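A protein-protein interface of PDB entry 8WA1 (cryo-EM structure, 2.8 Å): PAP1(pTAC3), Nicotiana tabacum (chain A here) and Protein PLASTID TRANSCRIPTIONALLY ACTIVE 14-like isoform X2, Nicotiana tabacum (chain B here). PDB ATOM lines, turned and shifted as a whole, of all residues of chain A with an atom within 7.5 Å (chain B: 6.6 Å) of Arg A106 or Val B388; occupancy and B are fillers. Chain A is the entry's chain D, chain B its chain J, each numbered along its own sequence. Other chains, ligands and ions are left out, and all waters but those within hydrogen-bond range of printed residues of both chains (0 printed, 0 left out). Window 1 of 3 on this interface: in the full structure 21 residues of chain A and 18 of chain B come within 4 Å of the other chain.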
ATOM      1  N   MET A  74      -0.760 -22.775  -9.836  1.00  0.00           N
ATOM      2  CA  MET A  74      -0.309 -22.196  -8.579  1.00  0.00           C
ATOM      3  C   MET A  74      -1.224 -22.556  -7.418  1.00  0.00           C
ATOM      4  O   MET A  74      -0.757 -22.603  -6.278  1.00  0.00           O
ATOM      5  CB  MET A  74      -0.208 -20.676  -8.714  1.00  0.00           C
ATOM      6  CG  MET A  74       0.528 -19.991  -7.575  1.00  0.00           C
ATOM      7  SD  MET A  74       2.297 -20.339  -7.588  1.00  0.00           S
ATOM      8  CE  MET A  74       2.767 -19.617  -9.158  1.00  0.00           C
ATOM      9  N   LEU A  77       0.103 -25.816  -6.396  1.00  0.00           N
ATOM     10  CA  LEU A  77       1.458 -25.594  -5.896  1.00  0.00           C
ATOM     11  C   LEU A  77       1.431 -25.064  -4.465  1.00  0.00           C
ATOM     12  O   LEU A  77       2.103 -25.601  -3.576  1.00  0.00           O
ATOM     13  CB  LEU A  77       2.212 -24.636  -6.820  1.00  0.00           C
ATOM     14  CG  LEU A  77       3.704 -24.441  -6.533  1.00  0.00           C
ATOM     15  CD1 LEU A  77       4.503 -24.451  -7.826  1.00  0.00           C
ATOM     16  CD2 LEU A  77       3.954 -23.149  -5.763  1.00  0.00           C
ATOM     17  N   MET A  78       0.638 -24.018  -4.221  1.00  0.00           N
ATOM     18  CA  MET A  78       0.547 -23.447  -2.883  1.00  0.00           C
ATOM     19  C   MET A  78      -0.132 -24.396  -1.907  1.00  0.00           C
ATOM     20  O   MET A  78       0.216 -24.410  -0.722  1.00  0.00           O
ATOM     21  CB  MET A  78      -0.196 -22.112  -2.932  1.00  0.00           C
ATOM     22  CG  MET A  78       0.555 -21.020  -3.670  1.00  0.00           C
ATOM     23  SD  MET A  78       2.200 -20.748  -2.985  1.00  0.00           S
ATOM     24  CE  MET A  78       2.799 -19.434  -4.043  1.00  0.00           C
ATOM     25  N   MET A  96       4.381 -27.845 -14.624  1.00  0.00           N
ATOM     26  CA  MET A  96       4.468 -26.537 -15.269  1.00  0.00           C
ATOM     27  C   MET A  96       5.508 -26.546 -16.380  1.00  0.00           C
ATOM     28  O   MET A  96       5.296 -25.960 -17.447  1.00  0.00           O
ATOM     29  CB  MET A  96       4.806 -25.454 -14.243  1.00  0.00           C
ATOM     30  CG  MET A  96       3.827 -25.335 -13.092  1.00  0.00           C
ATOM     31  SD  MET A  96       4.035 -23.794 -12.183  1.00  0.00           S
ATOM     32  CE  MET A  96       5.814 -23.763 -11.990  1.00  0.00           C
ATOM     33  N   PRO A 103       8.568 -21.658 -14.860  1.00  0.00           N
ATOM     34  CA  PRO A 103       8.493 -21.309 -13.439  1.00  0.00           C
ATOM     35  C   PRO A 103       8.956 -19.884 -13.183  1.00  0.00           C
ATOM     36  O   PRO A 103       9.586 -19.237 -14.024  1.00  0.00           O
ATOM     37  CB  PRO A 103       9.429 -22.324 -12.771  1.00  0.00           C
ATOM     38  CG  PRO A 103       9.555 -23.442 -13.761  1.00  0.00           C
ATOM     39  CD  PRO A 103       9.478 -22.788 -15.104  1.00  0.00           C
ATOM     40  N   GLY A 104       8.630 -19.397 -11.989  1.00  0.00           N
ATOM     41  CA  GLY A 104       8.973 -18.053 -11.595  1.00  0.00           C
ATOM     42  C   GLY A 104       9.464 -17.985 -10.164  1.00  0.00           C
ATOM     43  O   GLY A 104       9.581 -19.002  -9.474  1.00  0.00           O
ATOM     44  N   PRO A 105       9.764 -16.772  -9.690  1.00  0.00           N
ATOM     45  CA  PRO A 105      10.208 -16.613  -8.299  1.00  0.00           C
ATOM     46  C   PRO A 105       9.134 -17.015  -7.300  1.00  0.00           C
ATOM     47  O   PRO A 105       9.432 -17.331  -6.144  1.00  0.00           O
ATOM     48  CB  PRO A 105      10.536 -15.117  -8.206  1.00  0.00           C
ATOM     49  CG  PRO A 105       9.697 -14.485  -9.266  1.00  0.00           C
ATOM     50  CD  PRO A 105       9.657 -15.481 -10.390  1.00  0.00           C
ATOM     51  N   ARG A 106       7.877 -17.009  -7.746  1.00  0.00           N
ATOM     52  CA  ARG A 106       6.771 -17.414  -6.885  1.00  0.00           C
ATOM     53  C   ARG A 106       6.638 -18.928  -6.805  1.00  0.00           C
ATOM     54  O   ARG A 106       6.128 -19.449  -5.808  1.00  0.00           O
ATOM     55  CB  ARG A 106       5.465 -16.802  -7.390  1.00  0.00           C
ATOM     56  CG  ARG A 106       5.541 -15.308  -7.633  1.00  0.00           C
ATOM     57  CD  ARG A 106       5.621 -14.538  -6.328  1.00  0.00           C
ATOM     58  NE  ARG A 106       6.259 -13.237  -6.508  1.00  0.00           N
ATOM     59  CZ  ARG A 106       5.637 -12.157  -6.966  1.00  0.00           C
ATOM     60  NH1 ARG A 106       4.353 -12.216  -7.297  1.00  0.00           N
ATOM     61  NH2 ARG A 106       6.299 -11.016  -7.098  1.00  0.00           N
ATOM     62  N   SER A 107       7.077 -19.644  -7.842  1.00  0.00           N
ATOM     63  CA  SER A 107       6.982 -21.100  -7.825  1.00  0.00           C
ATOM     64  C   SER A 107       7.998 -21.706  -6.867  1.00  0.00           C
ATOM     65  O   SER A 107       7.643 -22.524  -6.010  1.00  0.00           O
ATOM     66  CB  SER A 107       7.177 -21.657  -9.234  1.00  0.00           C
ATOM     67  OG  SER A 107       7.219 -23.072  -9.213  1.00  0.00           O
ATOM     68  N   PHE A 108       9.269 -21.317  -6.995  1.00  0.00           N
ATOM     69  CA  PHE A 108      10.299 -21.828  -6.100  1.00  0.00           C
ATOM     70  C   PHE A 108      10.087 -21.379  -4.662  1.00  0.00           C
ATOM     71  O   PHE A 108      10.618 -22.014  -3.745  1.00  0.00           O
ATOM     72  CB  PHE A 108      11.684 -21.391  -6.582  1.00  0.00           C
ATOM     73  CG  PHE A 108      12.071 -21.971  -7.911  1.00  0.00           C
ATOM     74  CD1 PHE A 108      12.727 -23.188  -7.985  1.00  0.00           C
ATOM     75  CD2 PHE A 108      11.777 -21.301  -9.086  1.00  0.00           C
ATOM     76  CE1 PHE A 108      13.084 -23.726  -9.205  1.00  0.00           C
ATOM     77  CE2 PHE A 108      12.131 -21.833 -10.311  1.00  0.00           C
ATOM     78  CZ  PHE A 108      12.785 -23.048 -10.370  1.00  0.00           C
ATOM     79  N   HIS A 109       9.333 -20.299  -4.447  1.00  0.00           N
ATOM     80  CA  HIS A 109       8.975 -19.898  -3.090  1.00  0.00           C
ATOM     81  C   HIS A 109       8.200 -21.001  -2.380  1.00  0.00           C
ATOM     82  O   HIS A 109       8.445 -21.281  -1.199  1.00  0.00           O
ATOM     83  CB  HIS A 109       8.159 -18.605  -3.130  1.00  0.00           C
ATOM     84  CG  HIS A 109       7.334 -18.370  -1.905  1.00  0.00           C
ATOM     85  ND1 HIS A 109       7.877 -17.954  -0.708  1.00  0.00           N
ATOM     86  CD2 HIS A 109       6.002 -18.492  -1.690  1.00  0.00           C
ATOM     87  CE1 HIS A 109       6.915 -17.830   0.190  1.00  0.00           C
ATOM     88  NE2 HIS A 109       5.768 -18.151  -0.380  1.00  0.00           N
ATOM     89  N   GLY A 110       7.267 -21.641  -3.087  1.00  0.00           N
ATOM     90  CA  GLY A 110       6.528 -22.743  -2.495  1.00  0.00           C
ATOM     91  C   GLY A 110       7.420 -23.914  -2.135  1.00  0.00           C
ATOM     92  O   GLY A 110       7.278 -24.506  -1.063  1.00  0.00           O
ATOM     93  N   PHE A 111       8.354 -24.261  -3.021  1.00  0.00           N
ATOM     94  CA  PHE A 111       9.292 -25.341  -2.730  1.00  0.00           C
ATOM     95  C   PHE A 111      10.152 -25.005  -1.517  1.00  0.00           C
ATOM     96  O   PHE A 111      10.371 -25.850  -0.637  1.00  0.00           O
ATOM     97  CB  PHE A 111      10.166 -25.607  -3.957  1.00  0.00           C
ATOM     98  CG  PHE A 111      10.566 -27.045  -4.120  1.00  0.00           C
ATOM     99  CD1 PHE A 111      10.120 -28.008  -3.231  1.00  0.00           C
ATOM    100  CD2 PHE A 111      11.392 -27.433  -5.162  1.00  0.00           C
ATOM    101  CE1 PHE A 111      10.487 -29.333  -3.378  1.00  0.00           C
ATOM    102  CE2 PHE A 111      11.764 -28.755  -5.316  1.00  0.00           C
ATOM    103  CZ  PHE A 111      11.310 -29.706  -4.422  1.00  0.00           C
ATOM    104  N   GLU A 131      16.623 -22.352  -8.376  1.00  0.00           N
ATOM    105  CA  GLU A 131      16.009 -21.081  -8.746  1.00  0.00           C
ATOM    106  C   GLU A 131      17.048 -20.094  -9.267  1.00  0.00           C
ATOM    107  O   GLU A 131      16.785 -19.345 -10.214  1.00  0.00           O
ATOM    108  CB  GLU A 131      15.258 -20.492  -7.551  1.00  0.00           C
ATOM    109  CG  GLU A 131      14.531 -19.191  -7.857  1.00  0.00           C
ATOM    110  CD  GLU A 131      13.844 -18.603  -6.639  1.00  0.00           C
ATOM    111  OE1 GLU A 131      13.991 -19.175  -5.538  1.00  0.00           O
ATOM    112  OE2 GLU A 131      13.156 -17.571  -6.781  1.00  0.00           O
ATOM    113  N   LEU A 136      16.498 -16.417 -12.351  1.00  0.00           N
ATOM    114  CA  LEU A 136      15.521 -15.548 -11.711  1.00  0.00           C
ATOM    115  C   LEU A 136      16.017 -15.151 -10.329  1.00  0.00           C
ATOM    116  O   LEU A 136      16.487 -16.001  -9.565  1.00  0.00           O
ATOM    117  CB  LEU A 136      14.163 -16.245 -11.610  1.00  0.00           C
ATOM    118  CG  LEU A 136      13.633 -16.840 -12.916  1.00  0.00           C
ATOM    119  CD1 LEU A 136      12.373 -17.644 -12.661  1.00  0.00           C
ATOM    120  CD2 LEU A 136      13.378 -15.749 -13.943  1.00  0.00           C
ATOM    121  N   ARG A 137      15.913 -13.865 -10.014  1.00  0.00           N
ATOM    122  CA  ARG A 137      16.312 -13.385  -8.698  1.00  0.00           C
ATOM    123  C   ARG A 137      15.352 -13.919  -7.637  1.00  0.00           C
ATOM    124  O   ARG A 137      14.130 -13.791  -7.794  1.00  0.00           O
ATOM    125  CB  ARG A 137      16.333 -11.858  -8.670  1.00  0.00           C
ATOM    126  CG  ARG A 137      17.391 -11.236  -9.565  1.00  0.00           C
ATOM    127  CD  ARG A 137      17.194  -9.731  -9.714  1.00  0.00           C
ATOM    128  NE  ARG A 137      17.306  -9.015  -8.445  1.00  0.00           N
ATOM    129  CZ  ARG A 137      16.268  -8.586  -7.732  1.00  0.00           C
ATOM    130  NH1 ARG A 137      15.032  -8.799  -8.163  1.00  0.00           N
ATOM    131  NH2 ARG A 137      16.465  -7.943  -6.591  1.00  0.00           N
ATOM    132  N   LEU A 139      13.061 -14.252  -4.276  1.00  0.00           N
ATOM    133  CA  LEU A 139      12.263 -13.287  -3.537  1.00  0.00           C
ATOM    134  C   LEU A 139      12.856 -13.038  -2.153  1.00  0.00           C
ATOM    135  O   LEU A 139      13.631 -13.840  -1.621  1.00  0.00           O
ATOM    136  CB  LEU A 139      10.821 -13.773  -3.401  1.00  0.00           C
ATOM    137  CG  LEU A 139      10.048 -14.010  -4.697  1.00  0.00           C
ATOM    138  CD1 LEU A 139       8.654 -14.528  -4.391  1.00  0.00           C
ATOM    139  CD2 LEU A 139       9.981 -12.734  -5.523  1.00  0.00           C
ATOM    140  N   THR A 142      11.830 -15.747   0.393  1.00  0.00           N
ATOM    141  CA  THR A 142      12.627 -16.971   0.368  1.00  0.00           C
ATOM    142  C   THR A 142      13.882 -16.823   1.219  1.00  0.00           C
ATOM    143  O   THR A 142      14.196 -17.691   2.045  1.00  0.00           O
ATOM    144  CB  THR A 142      12.996 -17.323  -1.074  1.00  0.00           C
ATOM    145  OG1 THR A 142      11.813 -17.674  -1.803  1.00  0.00           O
ATOM    146  CG2 THR A 142      13.977 -18.483  -1.108  1.00  0.00           C
ATOM    147  N   ASP B 383       3.481  -9.431   3.295  1.00  0.00           N
ATOM    148  CA  ASP B 383       4.797  -9.723   2.738  1.00  0.00           C
ATOM    149  C   ASP B 383       4.761  -9.817   1.220  1.00  0.00           C
ATOM    150  O   ASP B 383       5.606  -9.217   0.545  1.00  0.00           O
ATOM    151  CB  ASP B 383       5.348 -11.019   3.333  1.00  0.00           C
ATOM    152  CG  ASP B 383       6.790 -11.282   2.930  1.00  0.00           C
ATOM    153  OD1 ASP B 383       7.043 -11.600   1.747  1.00  0.00           O
ATOM    154  OD2 ASP B 383       7.677 -11.156   3.799  1.00  0.00           O
ATOM    155  N   THR B 384       3.792 -10.549   0.669  1.00  0.00           N
ATOM    156  CA  THR B 384       3.699 -10.673  -0.782  1.00  0.00           C
ATOM    157  C   THR B 384       3.375  -9.331  -1.425  1.00  0.00           C
ATOM    158  O   THR B 384       3.850  -9.034  -2.527  1.00  0.00           O
ATOM    159  CB  THR B 384       2.647 -11.720  -1.149  1.00  0.00           C
ATOM    160  OG1 THR B 384       2.940 -12.946  -0.468  1.00  0.00           O
ATOM    161  CG2 THR B 384       2.644 -11.973  -2.648  1.00  0.00           C
ATOM    162  N   PHE B 385       2.580  -8.502  -0.746  1.00  0.00           N
ATOM    163  CA  PHE B 385       2.277  -7.169  -1.255  1.00  0.00           C
ATOM    164  C   PHE B 385       3.536  -6.316  -1.345  1.00  0.00           C
ATOM    165  O   PHE B 385       3.823  -5.716  -2.391  1.00  0.00           O
ATOM    166  CB  PHE B 385       1.233  -6.509  -0.352  1.00  0.00           C
ATOM    167  CG  PHE B 385       0.541  -5.332  -0.971  1.00  0.00           C
ATOM    168  CD1 PHE B 385      -0.411  -5.514  -1.961  1.00  0.00           C
ATOM    169  CD2 PHE B 385       0.830  -4.046  -0.554  1.00  0.00           C
ATOM    170  CE1 PHE B 385      -1.056  -4.433  -2.527  1.00  0.00           C
ATOM    171  CE2 PHE B 385       0.186  -2.961  -1.116  1.00  0.00           C
ATOM    172  CZ  PHE B 385      -0.756  -3.155  -2.106  1.00  0.00           C
ATOM    173  N   LEU B 386       4.308  -6.259  -0.256  1.00  0.00           N
ATOM    174  CA  LEU B 386       5.546  -5.486  -0.267  1.00  0.00           C
ATOM    175  C   LEU B 386       6.544  -6.059  -1.266  1.00  0.00           C
ATOM    176  O   LEU B 386       7.368  -5.323  -1.822  1.00  0.00           O
ATOM    177  CB  LEU B 386       6.154  -5.444   1.135  1.00  0.00           C
ATOM    178  CG  LEU B 386       5.272  -4.890   2.258  1.00  0.00           C
ATOM    179  CD1 LEU B 386       6.047  -4.821   3.564  1.00  0.00           C
ATOM    180  CD2 LEU B 386       4.702  -3.530   1.889  1.00  0.00           C
ATOM    181  N   SER B 387       6.491  -7.372  -1.502  1.00  0.00           N
ATOM    182  CA  SER B 387       7.388  -7.981  -2.479  1.00  0.00           C
ATOM    183  C   SER B 387       7.015  -7.581  -3.900  1.00  0.00           C
ATOM    184  O   SER B 387       7.879  -7.162  -4.680  1.00  0.00           O
ATOM    185  CB  SER B 387       7.372  -9.503  -2.332  1.00  0.00           C
ATOM    186  OG  SER B 387       7.799  -9.898  -1.040  1.00  0.00           O
ATOM    187  N   VAL B 388       5.735  -7.711  -4.259  1.00  0.00           N
ATOM    188  CA  VAL B 388       5.314  -7.394  -5.621  1.00  0.00           C
ATOM    189  C   VAL B 388       5.447  -5.901  -5.887  1.00  0.00           C
ATOM    190  O   VAL B 388       5.637  -5.477  -7.033  1.00  0.00           O
ATOM    191  CB  VAL B 388       3.878  -7.892  -5.878  1.00  0.00           C
ATOM    192  CG1 VAL B 388       3.791  -9.397  -5.668  1.00  0.00           C
ATOM    193  CG2 VAL B 388       2.877  -7.161  -4.998  1.00  0.00           C
ATOM    194  N   PHE B 389       5.352  -5.078  -4.842  1.00  0.00           N
ATOM    195  CA  PHE B 389       5.500  -3.637  -4.990  1.00  0.00           C
ATOM    196  C   PHE B 389       6.870  -3.136  -4.549  1.00  0.00           C
ATOM    197  O   PHE B 389       7.088  -1.920  -4.495  1.00  0.00           O
ATOM    198  CB  PHE B 389       4.391  -2.914  -4.233  1.00  0.00           C
ATOM    199  CG  PHE B 389       3.077  -2.907  -4.956  1.00  0.00           C
ATOM    200  CD1 PHE B 389       2.883  -2.075  -6.046  1.00  0.00           C
ATOM    201  CD2 PHE B 389       2.041  -3.731  -4.555  1.00  0.00           C
ATOM    202  CE1 PHE B 389       1.681  -2.066  -6.722  1.00  0.00           C
ATOM    203  CE2 PHE B 389       0.836  -3.726  -5.229  1.00  0.00           C
ATOM    204  CZ  PHE B 389       0.656  -2.892  -6.312  1.00  0.00           C
ATOM    205  N   ASN B 390       7.794  -4.049  -4.252  1.00  0.00           N
ATOM    206  CA  ASN B 390       9.189  -3.718  -3.953  1.00  0.00           C
ATOM    207  C   ASN B 390       9.296  -2.666  -2.850  1.00  0.00           C
ATOM    208  O   ASN B 390       9.909  -1.609  -3.018  1.00  0.00           O
ATOM    209  CB  ASN B 390       9.919  -3.262  -5.216  1.00  0.00           C
ATOM    210  CG  ASN B 390       9.973  -4.342  -6.280  1.00  0.00           C
ATOM    211  OD1 ASN B 390       9.502  -4.149  -7.400  1.00  0.00           O
ATOM    212  ND2 ASN B 390      10.546  -5.487  -5.933  1.00  0.00           N
ATOM    213  N   ILE B 391       8.688  -2.965  -1.708  1.00  0.00           N
ATOM    214  CA  ILE B 391       8.776  -2.130  -0.517  1.00  0.00           C
ATOM    215  C   ILE B 391       9.662  -2.844   0.493  1.00  0.00           C
ATOM    216  O   ILE B 391       9.428  -4.014   0.815  1.00  0.00           O
ATOM    217  CB  ILE B 391       7.385  -1.832   0.069  1.00  0.00           C
ATOM    218  CG1 ILE B 391       6.529  -1.089  -0.959  1.00  0.00           C
ATOM    219  CG2 ILE B 391       7.508  -1.023   1.350  1.00  0.00           C
ATOM    220  CD1 ILE B 391       5.139  -0.753  -0.469  1.00  0.00           C
ATOM    221  N   ASP B 409       8.906   0.391 -13.057  1.00  0.00           N
ATOM    222  CA  ASP B 409       7.831   0.703 -12.124  1.00  0.00           C
ATOM    223  C   ASP B 409       7.944   2.058 -11.470  1.00  0.00           C
ATOM    224  O   ASP B 409       8.831   2.288 -10.655  1.00  0.00           O
ATOM    225  CB  ASP B 409       7.734  -0.372 -11.039  1.00  0.00           C
ATOM    226  CG  ASP B 409       6.403  -0.345 -10.312  1.00  0.00           C
ATOM    227  OD1 ASP B 409       5.370  -0.128 -10.977  1.00  0.00           O
ATOM    228  OD2 ASP B 409       6.389  -0.544  -9.080  1.00  0.00           O
ATOM    229  N   ALA B 497      -3.746  -0.787  -7.225  1.00  0.00           N
ATOM    230  CA  ALA B 497      -2.681  -1.559  -6.597  1.00  0.00           C
ATOM    231  C   ALA B 497      -3.166  -2.947  -6.204  1.00  0.00           C
ATOM    232  O   ALA B 497      -2.431  -3.929  -6.343  1.00  0.00           O
ATOM    233  CB  ALA B 497      -2.138  -0.814  -5.378  1.00  0.00           C
ATOM    234  N   ILE B 500      -3.224  -4.902  -9.421  1.00  0.00           N
ATOM    235  CA  ILE B 500      -1.872  -5.281  -9.821  1.00  0.00           C
ATOM    236  C   ILE B 500      -1.341  -6.400  -8.936  1.00  0.00           C
ATOM    237  O   ILE B 500      -0.632  -7.294  -9.412  1.00  0.00           O
ATOM    238  CB  ILE B 500      -0.945  -4.047  -9.798  1.00  0.00           C
ATOM    239  CG1 ILE B 500      -1.353  -3.055 -10.888  1.00  0.00           C
ATOM    240  CG2 ILE B 500       0.509  -4.454  -9.978  1.00  0.00           C
ATOM    241  CD1 ILE B 500      -0.504  -1.802 -10.924  1.00  0.00           C
ATOM    242  N   TYR B 501      -1.671  -6.375  -7.644  1.00  0.00           N
ATOM    243  CA  TYR B 501      -1.278  -7.464  -6.755  1.00  0.00           C
ATOM    244  C   TYR B 501      -1.938  -8.774  -7.169  1.00  0.00           C
ATOM    245  O   TYR B 501      -1.274  -9.814  -7.254  1.00  0.00           O
ATOM    246  CB  TYR B 501      -1.636  -7.107  -5.312  1.00  0.00           C
ATOM    247  CG  TYR B 501      -1.465  -8.233  -4.317  1.00  0.00           C
ATOM    248  CD1 TYR B 501      -0.242  -8.466  -3.706  1.00  0.00           C
ATOM    249  CD2 TYR B 501      -2.534  -9.054  -3.979  1.00  0.00           C
ATOM    250  CE1 TYR B 501      -0.085  -9.490  -2.792  1.00  0.00           C
ATOM    251  CE2 TYR B 501      -2.385 -10.080  -3.069  1.00  0.00           C
ATOM    252  CZ  TYR B 501      -1.159 -10.293  -2.477  1.00  0.00           C
ATOM    253  OH  TYR B 501      -1.008 -11.314  -1.568  1.00  0.00           O
ATOM    254  N   ARG B 504      -0.087  -9.934 -10.373  1.00  0.00           N
ATOM    255  CA  ARG B 504       1.320 -10.322 -10.309  1.00  0.00           C
ATOM    256  C   ARG B 504       1.557 -11.470  -9.336  1.00  0.00           C
ATOM    257  O   ARG B 504       2.586 -12.150  -9.428  1.00  0.00           O
ATOM    258  CB  ARG B 504       2.173  -9.112  -9.929  1.00  0.00           C
ATOM    259  CG  ARG B 504       3.647  -9.255 -10.263  1.00  0.00           C
ATOM    260  CD  ARG B 504       4.322  -7.895 -10.309  1.00  0.00           C
ATOM    261  NE  ARG B 504       3.719  -7.030 -11.319  1.00  0.00           N
ATOM    262  CZ  ARG B 504       4.102  -5.782 -11.564  1.00  0.00           C
ATOM    263  NH1 ARG B 504       5.094  -5.241 -10.872  1.00  0.00           N
ATOM    264  NH2 ARG B 504       3.491  -5.073 -12.504  1.00  0.00           N
ATOM    265  N   ILE B 505       0.633 -11.700  -8.398  1.00  0.00           N
ATOM    266  CA  ILE B 505       0.804 -12.799  -7.450  1.00  0.00           C
ATOM    267  C   ILE B 505       0.858 -14.136  -8.182  1.00  0.00           C
ATOM    268  O   ILE B 505       1.503 -15.087  -7.724  1.00  0.00           O
ATOM    269  CB  ILE B 505      -0.315 -12.771  -6.390  1.00  0.00           C
ATOM    270  CG1 ILE B 505      -0.011 -13.753  -5.256  1.00  0.00           C
ATOM    271  CG2 ILE B 505      -1.668 -13.083  -7.014  1.00  0.00           C
ATOM    272  CD1 ILE B 505      -1.069 -13.780  -4.175  1.00  0.00           C
ATOM    273  N   LEU B 506       0.196 -14.225  -9.337  1.00  0.00           N
ATOM    274  CA  LEU B 506       0.191 -15.448 -10.142  1.00  0.00           C
ATOM    275  C   LEU B 506       1.198 -15.312 -11.286  1.00  0.00           C
ATOM    276  O   LEU B 506       0.882 -14.903 -12.404  1.00  0.00           O
ATOM    277  CB  LEU B 506      -1.212 -15.739 -10.656  1.00  0.00           C
ATOM    278  CG  LEU B 506      -2.253 -16.025  -9.575  1.00  0.00           C
ATOM    279  CD1 LEU B 506      -3.629 -16.228 -10.186  1.00  0.00           C
ATOM    280  CD2 LEU B 506      -1.841 -17.238  -8.758  1.00  0.00           C
ATOM    281  N   PHE B 507       2.441 -15.659 -10.973  1.00  0.00           N
ATOM    282  CA  PHE B 507       3.515 -15.623 -11.958  1.00  0.00           C
ATOM    283  C   PHE B 507       4.207 -16.979 -12.053  1.00  0.00           C
ATOM    284  O   PHE B 507       4.324 -17.551 -13.136  1.00  0.00           O
ATOM    285  CB  PHE B 507       4.530 -14.532 -11.609  1.00  0.00           C
ATOM    286  CG  PHE B 507       5.580 -14.320 -12.663  1.00  0.00           C
ATOM    287  CD1 PHE B 507       5.340 -13.477 -13.736  1.00  0.00           C
ATOM    288  CD2 PHE B 507       6.806 -14.959 -12.581  1.00  0.00           C
ATOM    289  CE1 PHE B 507       6.302 -13.278 -14.708  1.00  0.00           C
ATOM    290  CE2 PHE B 507       7.773 -14.763 -13.550  1.00  0.00           C
ATOM    291  CZ  PHE B 507       7.519 -13.921 -14.615  1.00  0.00           C
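The backbone carbonyl oxygen of Arg B504 sits at hydrogen-bond distance from the guanidinium group of Arg A106, at 2.8 Å.
Met A74 touches Leu B506 (CB to CD2, 3.8 Å).
Gly A104 touches Phe B507 (CA to CD2, 3.9 Å).
CD2 of Phe B507 touches CD of Pro A105 (3.6 Å).
CG1 of Val B388 touches NH1 of Arg A106, 3.3 Å away.
Ile B505 touches Arg A106 (CA to NH1, 3.6 Å).
Arg A106 touches just these residues of chain B: Val B388 (3.3 Å), Arg B504 (2.8 Å) and Ile B505 (3.6 Å).
Leu B386 touches none of the printed residues of chain A.
Val B388 touches one residue of chain A.
Ile B391 touches none of the printed residues of chain A.
Of the printed residues of chain A, Arg B504 touches Arg A106 (2.8 Å).
Of the printed residues of chain A, Phe B507 touches Gly A104 (3.9 Å) and Pro A105 (3.6 Å).
The nearest residue of chain B that does not touch Arg A106 is Phe B507 (4.2 Å).
The nearest printed residue of chain B that does not touch Met A74 is Phe B507 (4.2 Å).
Hydrophobic or aromatic side chains of chain A that line the printed part of chain B: Met A74 and Pro A105.
Of the 17 printed residues of chain B, 5 touch a printed residue of chain A.
Hydrophobic or aromatic side chains of chain B that line the printed part of chain A: Val B388, Leu B506 and Phe B507.
Among the printed residues, no Asp or Glu carboxylate lies within 4 Å of a Lys or Arg side-chain nitrogen of the other chain.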
